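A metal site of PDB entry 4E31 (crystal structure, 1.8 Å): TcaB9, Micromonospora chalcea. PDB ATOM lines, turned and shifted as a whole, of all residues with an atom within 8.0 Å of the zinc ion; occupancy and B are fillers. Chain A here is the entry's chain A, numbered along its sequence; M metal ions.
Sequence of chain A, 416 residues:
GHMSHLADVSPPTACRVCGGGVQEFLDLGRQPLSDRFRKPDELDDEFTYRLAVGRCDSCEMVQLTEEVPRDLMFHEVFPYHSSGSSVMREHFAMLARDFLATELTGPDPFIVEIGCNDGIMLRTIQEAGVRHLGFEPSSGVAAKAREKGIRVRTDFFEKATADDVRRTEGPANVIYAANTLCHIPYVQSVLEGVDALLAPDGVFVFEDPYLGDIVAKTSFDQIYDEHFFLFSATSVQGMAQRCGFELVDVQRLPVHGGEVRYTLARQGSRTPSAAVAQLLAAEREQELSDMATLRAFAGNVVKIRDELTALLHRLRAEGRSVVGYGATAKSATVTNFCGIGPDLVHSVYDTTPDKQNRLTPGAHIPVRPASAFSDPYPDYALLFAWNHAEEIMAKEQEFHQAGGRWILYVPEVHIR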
ATOM      1  N   ALA A  14     -17.208   4.099  -1.459  1.00  0.00           N
ATOM      2  CA  ALA A  14     -16.200   5.164  -1.426  1.00  0.00           C
ATOM      3  C   ALA A  14     -14.801   4.621  -1.122  1.00  0.00           C
ATOM      4  O   ALA A  14     -14.642   3.878  -0.149  1.00  0.00           O
ATOM      5  CB  ALA A  14     -16.536   6.227  -0.383  1.00  0.00           C
ATOM      6  N   CYS A  15     -13.800   5.014  -1.906  1.00  0.00           N
ATOM      7  CA  CYS A  15     -12.395   4.710  -1.596  1.00  0.00           C
ATOM      8  C   CYS A  15     -11.994   5.083  -0.176  1.00  0.00           C
ATOM      9  O   CYS A  15     -12.230   6.207   0.251  1.00  0.00           O
ATOM     10  CB  CYS A  15     -11.463   5.442  -2.554  1.00  0.00           C
ATOM     11  SG  CYS A  15      -9.718   5.080  -2.269  1.00  0.00           S
ATOM     12  N   ARG A  16     -11.398   4.128   0.549  1.00  0.00           N
ATOM     13  CA  ARG A  16     -10.925   4.365   1.915  1.00  0.00           C
ATOM     14  C   ARG A  16      -9.660   5.228   2.054  1.00  0.00           C
ATOM     15  O   ARG A  16      -9.343   5.703   3.156  1.00  0.00           O
ATOM     16  CB  ARG A  16     -10.783   3.032   2.680  1.00  0.00           C
ATOM     17  CG  ARG A  16     -12.090   2.493   3.205  1.00  0.00           C
ATOM     18  CD  ARG A  16     -12.587   3.426   4.332  1.00  0.00           C
ATOM     19  NE  ARG A  16     -12.933   2.647   5.510  1.00  0.00           N
ATOM     20  CZ  ARG A  16     -12.695   2.982   6.771  1.00  0.00           C
ATOM     21  NH1 ARG A  16     -13.077   2.158   7.722  1.00  0.00           N
ATOM     22  NH2 ARG A  16     -12.112   4.129   7.111  1.00  0.00           N
ATOM     23  N   VAL A  17      -8.980   5.454   0.946  1.00  0.00           N
ATOM     24  CA  VAL A  17      -7.822   6.332   0.912  1.00  0.00           C
ATOM     25  C   VAL A  17      -8.246   7.773   0.620  1.00  0.00           C
ATOM     26  O   VAL A  17      -7.884   8.653   1.411  1.00  0.00           O
ATOM     27  CB  VAL A  17      -6.728   5.804  -0.039  1.00  0.00           C
ATOM     28  CG1 VAL A  17      -5.589   6.804  -0.172  1.00  0.00           C
ATOM     29  CG2 VAL A  17      -6.228   4.519   0.583  1.00  0.00           C
ATOM     30  N   CYS A  18      -8.988   7.983  -0.457  1.00  0.00           N
ATOM     31  CA  CYS A  18      -9.200   9.345  -0.943  1.00  0.00           C
ATOM     32  C   CYS A  18     -10.672   9.736  -1.132  1.00  0.00           C
ATOM     33  O   CYS A  18     -10.949  10.857  -1.546  1.00  0.00           O
ATOM     34  CB  CYS A  18      -8.485   9.571  -2.263  1.00  0.00           C
ATOM     35  SG  CYS A  18      -9.406   8.844  -3.635  1.00  0.00           S
ATOM     36  N   GLY A  19     -11.581   8.805  -0.887  1.00  0.00           N
ATOM     37  CA  GLY A  19     -13.011   9.078  -1.054  1.00  0.00           C
ATOM     38  C   GLY A  19     -13.524   9.141  -2.491  1.00  0.00           C
ATOM     39  O   GLY A  19     -14.724   9.358  -2.655  1.00  0.00           O
ATOM     40  N   GLY A  20     -12.680   8.922  -3.503  1.00  0.00           N
ATOM     41  CA  GLY A  20     -13.110   8.743  -4.881  1.00  0.00           C
ATOM     42  C   GLY A  20     -14.046   7.557  -5.080  1.00  0.00           C
ATOM     43  O   GLY A  20     -14.325   6.843  -4.110  1.00  0.00           O
ATOM     44  N   GLY A  21     -14.554   7.317  -6.286  1.00  0.00           N
ATOM     45  CA  GLY A  21     -15.463   6.198  -6.525  1.00  0.00           C
ATOM     46  C   GLY A  21     -14.737   4.892  -6.798  1.00  0.00           C
ATOM     47  O   GLY A  21     -13.747   4.875  -7.547  1.00  0.00           O
ATOM     48  N   VAL A  22     -15.242   3.783  -6.238  1.00  0.00           N
ATOM     49  CA  VAL A  22     -14.600   2.483  -6.468  1.00  0.00           C
ATOM     50  C   VAL A  22     -15.368   1.704  -7.537  1.00  0.00           C
ATOM     51  O   VAL A  22     -16.574   1.536  -7.386  1.00  0.00           O
ATOM     52  CB  VAL A  22     -14.429   1.646  -5.165  1.00  0.00           C
ATOM     53  CG1 VAL A  22     -13.850   0.276  -5.457  1.00  0.00           C
ATOM     54  CG2 VAL A  22     -13.509   2.339  -4.145  1.00  0.00           C
ATOM     55  N   ARG A  55     -11.448  -0.771  -8.066  1.00  0.00           N
ATOM     56  CA  ARG A  55     -10.298   0.108  -8.106  1.00  0.00           C
ATOM     57  C   ARG A  55     -10.878   1.503  -7.972  1.00  0.00           C
ATOM     58  O   ARG A  55     -11.876   1.809  -8.630  1.00  0.00           O
ATOM     59  CB  ARG A  55      -9.580  -0.078  -9.459  1.00  0.00           C
ATOM     60  CG  ARG A  55      -8.332   0.796  -9.428  1.00  0.00           C
ATOM     61  CD  ARG A  55      -7.955   1.260 -10.824  1.00  0.00           C
ATOM     62  NE  ARG A  55      -8.845   2.319 -11.278  1.00  0.00           N
ATOM     63  CZ  ARG A  55      -8.841   2.810 -12.513  1.00  0.00           C
ATOM     64  NH1 ARG A  55      -9.717   3.752 -12.808  1.00  0.00           N
ATOM     65  NH2 ARG A  55      -7.993   2.343 -13.428  1.00  0.00           N
ATOM     66  N   CYS A  56     -10.272   2.298  -7.102  1.00  0.00           N
ATOM     67  CA  CYS A  56     -10.683   3.698  -7.023  1.00  0.00           C
ATOM     68  C   CYS A  56     -10.391   4.483  -8.294  1.00  0.00           C
ATOM     69  O   CYS A  56      -9.306   4.386  -8.885  1.00  0.00           O
ATOM     70  CB  CYS A  56     -10.008   4.368  -5.820  1.00  0.00           C
ATOM     71  SG  CYS A  56     -10.214   6.174  -5.747  1.00  0.00           S
ATOM     72  N   ASP A  57     -11.384   5.252  -8.704  1.00  0.00           N
ATOM     73  CA  ASP A  57     -11.303   6.230  -9.796  1.00  0.00           C
ATOM     74  C   ASP A  57     -10.228   7.304  -9.682  1.00  0.00           C
ATOM     75  O   ASP A  57      -9.756   7.798 -10.699  1.00  0.00           O
ATOM     76  CB  ASP A  57     -12.599   7.029  -9.853  1.00  0.00           C
ATOM     77  CG  ASP A  57     -13.678   6.248 -10.533  1.00  0.00           C
ATOM     78  OD1 ASP A  57     -13.258   5.297 -11.232  1.00  0.00           O
ATOM     79  OD2 ASP A  57     -14.857   6.620 -10.313  1.00  0.00           O
ATOM     80  N   SER A  58      -9.834   7.689  -8.482  1.00  0.00           N
ATOM     81  CA  SER A  58      -8.984   8.873  -8.368  1.00  0.00           C
ATOM     82  C   SER A  58      -7.541   8.556  -8.012  1.00  0.00           C
ATOM     83  O   SER A  58      -6.645   9.253  -8.467  1.00  0.00           O
ATOM     84  CB  SER A  58      -9.566   9.799  -7.297  1.00  0.00           C
ATOM     85  OG  SER A  58     -10.911  10.052  -7.645  1.00  0.00           O
ATOM     86  N   CYS A  59      -7.324   7.527  -7.187  1.00  0.00           N
ATOM     87  CA  CYS A  59      -5.993   7.266  -6.674  1.00  0.00           C
ATOM     88  C   CYS A  59      -5.460   5.906  -7.120  1.00  0.00           C
ATOM     89  O   CYS A  59      -4.329   5.535  -6.797  1.00  0.00           O
ATOM     90  CB  CYS A  59      -5.972   7.488  -5.168  1.00  0.00           C
ATOM     91  SG  CYS A  59      -6.712   6.026  -4.387  1.00  0.00           S
ATOM     92  N   GLU A  60      -6.265   5.167  -7.867  1.00  0.00           N
ATOM     93  CA  GLU A  60      -5.885   3.838  -8.356  1.00  0.00           C
ATOM     94  C   GLU A  60      -5.717   2.700  -7.340  1.00  0.00           C
ATOM     95  O   GLU A  60      -5.285   1.591  -7.705  1.00  0.00           O
ATOM     96  CB  GLU A  60      -4.723   3.838  -9.360  1.00  0.00           C
ATOM     97  CG  GLU A  60      -5.150   4.669 -10.562  1.00  0.00           C
ATOM     98  CD  GLU A  60      -3.944   4.869 -11.451  1.00  0.00           C
ATOM     99  OE1 GLU A  60      -3.733   3.942 -12.254  1.00  0.00           O
ATOM    100  OE2 GLU A  60      -3.242   5.892 -11.308  1.00  0.00           O
ATOM    101  N   MET A  61      -6.111   2.995  -6.106  1.00  0.00           N
ATOM    102  CA  MET A  61      -6.077   1.961  -5.077  1.00  0.00           C
ATOM    103  C   MET A  61      -7.093   0.844  -5.325  1.00  0.00           C
ATOM    104  O   MET A  61      -8.318   1.046  -5.409  1.00  0.00           O
ATOM    105  CB  MET A  61      -6.329   2.543  -3.674  1.00  0.00           C
ATOM    106  CG  MET A  61      -6.200   1.510  -2.553  1.00  0.00           C
ATOM    107  SD  MET A  61      -4.516   0.852  -2.362  1.00  0.00           S
ATOM    108  CE  MET A  61      -3.673   2.230  -1.573  1.00  0.00           C
ATOM    109  N   VAL A  62      -6.572  -0.379  -5.414  1.00  0.00           N
ATOM    110  CA  VAL A  62      -7.408  -1.567  -5.530  1.00  0.00           C
ATOM    111  C   VAL A  62      -7.775  -2.045  -4.134  1.00  0.00           C
ATOM    112  O   VAL A  62      -6.906  -2.232  -3.268  1.00  0.00           O
ATOM    113  CB  VAL A  62      -6.590  -2.640  -6.260  1.00  0.00           C
ATOM    114  CG1 VAL A  62      -7.296  -4.009  -6.184  1.00  0.00           C
ATOM    115  CG2 VAL A  62      -6.353  -2.166  -7.719  1.00  0.00           C
ATOM    116  N   GLN A  63      -9.057  -2.297  -3.901  1.00  0.00           N
ATOM    117  CA  GLN A  63      -9.563  -2.580  -2.566  1.00  0.00           C
ATOM    118  C   GLN A  63     -10.876  -3.352  -2.626  1.00  0.00           C
ATOM    119  O   GLN A  63     -11.575  -3.286  -3.654  1.00  0.00           O
ATOM    120  CB  GLN A  63      -9.767  -1.247  -1.826  1.00  0.00           C
ATOM    121  CG  GLN A  63     -10.954  -0.406  -2.300  1.00  0.00           C
ATOM    122  CD  GLN A  63     -10.671   1.039  -1.959  1.00  0.00           C
ATOM    123  OE1 GLN A  63     -11.072   1.533  -0.892  1.00  0.00           O
ATOM    124  NE2 GLN A  63      -9.859   1.692  -2.792  1.00  0.00           N
ATOM    125  N   PHE A 229      -6.753  -4.250   0.909  1.00  0.00           N
ATOM    126  CA  PHE A 229      -6.049  -3.559  -0.174  1.00  0.00           C
ATOM    127  C   PHE A 229      -5.082  -4.450  -0.930  1.00  0.00           C
ATOM    128  O   PHE A 229      -4.403  -5.283  -0.339  1.00  0.00           O
ATOM    129  CB  PHE A 229      -5.190  -2.428   0.431  1.00  0.00           C
ATOM    130  CG  PHE A 229      -5.993  -1.296   0.986  1.00  0.00           C
ATOM    131  CD1 PHE A 229      -6.825  -0.483   0.194  1.00  0.00           C
ATOM    132  CD2 PHE A 229      -5.939  -1.044   2.356  1.00  0.00           C
ATOM    133  CE1 PHE A 229      -7.553   0.558   0.832  1.00  0.00           C
ATOM    134  CE2 PHE A 229      -6.651  -0.015   2.971  1.00  0.00           C
ATOM    135  CZ  PHE A 229      -7.471   0.787   2.193  1.00  0.00           C
ATOM    136  N   SER A 235      -0.439   3.199  -6.300  1.00  0.00           N
ATOM    137  CA  SER A 235      -1.455   3.579  -5.315  1.00  0.00           C
ATOM    138  C   SER A 235      -0.812   3.957  -3.978  1.00  0.00           C
ATOM    139  O   SER A 235      -1.279   4.867  -3.292  1.00  0.00           O
ATOM    140  CB  SER A 235      -2.481   2.450  -5.105  1.00  0.00           C
ATOM    141  OG  SER A 235      -1.884   1.197  -4.786  1.00  0.00           O
ATOM    142  N   MET A 239      -1.236   7.405  -1.961  1.00  0.00           N
ATOM    143  CA  MET A 239      -1.725   7.407  -0.595  1.00  0.00           C
ATOM    144  C   MET A 239      -0.705   8.073   0.323  1.00  0.00           C
ATOM    145  O   MET A 239      -1.041   8.784   1.264  1.00  0.00           O
ATOM    146  CB  MET A 239      -1.894   5.947  -0.194  1.00  0.00           C
ATOM    147  CG  MET A 239      -2.025   5.685   1.300  1.00  0.00           C
ATOM    148  SD  MET A 239      -2.299   3.941   1.768  1.00  0.00           S
ATOM    149  CE  MET A 239      -0.640   3.286   1.809  1.00  0.00           C
ATOM    150  N   ARG A 242      -0.777  11.963  -0.203  1.00  0.00           N
ATOM    151  CA  ARG A 242      -1.948  12.647   0.316  1.00  0.00           C
ATOM    152  C   ARG A 242      -1.870  12.839   1.824  1.00  0.00           C
ATOM    153  O   ARG A 242      -2.589  13.680   2.330  1.00  0.00           O
ATOM    154  CB  ARG A 242      -3.239  11.904  -0.031  1.00  0.00           C
ATOM    155  CG  ARG A 242      -3.690  11.975  -1.481  1.00  0.00           C
ATOM    156  CD  ARG A 242      -4.715  10.854  -1.669  1.00  0.00           C
ATOM    157  NE  ARG A 242      -5.494  11.095  -2.891  1.00  0.00           N
ATOM    158  CZ  ARG A 242      -5.123  10.796  -4.128  1.00  0.00           C
ATOM    159  NH1 ARG A 242      -5.964  11.082  -5.126  1.00  0.00           N
ATOM    160  NH2 ARG A 242      -3.951  10.212  -4.380  1.00  0.00           N
HETATM  161 ZN    ZN M   1      -8.856   6.549  -3.887  1.00  0.00          ZN
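The backbone NH (N) of Cys 56 sits at hydrogen-bond distance from the backbone carbonyl oxygen (O) of Met 61 (2.9 Å). The backbone NH (N) of Cys 15 is in hydrogen-bond range of the backbone carbonyl oxygen (O) of Gly 20, at 2.9 Å. The side-chain sulfur (SG) of Cys 59 lies close to the backbone NH (N) of Met 61. The side-chain sulfur of Cys 56 lies close to the backbone NH of Ser 58 (3.1 Å). The side-chain sulfur of Cys 18 sits close to the backbone NH of Gly 20. N of Val 17 sits close to SG of Cys 15, 3.3 Å away. The side-chain amide nitrogen (NE2) of Gln 63 sits close to the side-chain sulfur (SG) of Cys 15 (3.4 Å).
The nearest printed residue that does not touch the zinc ion is Val 17 (4.5 Å).
SG of Cys 59 binds the zinc ion. The side-chain sulfur (SG) of Cys 56 binds the zinc ion (2.3 Å). SG of Cys 15 is bound to the zinc ion (2.3 Å). The side-chain sulfur (SG) of Cys 18 binds the zinc ion, 2.4 Å away.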
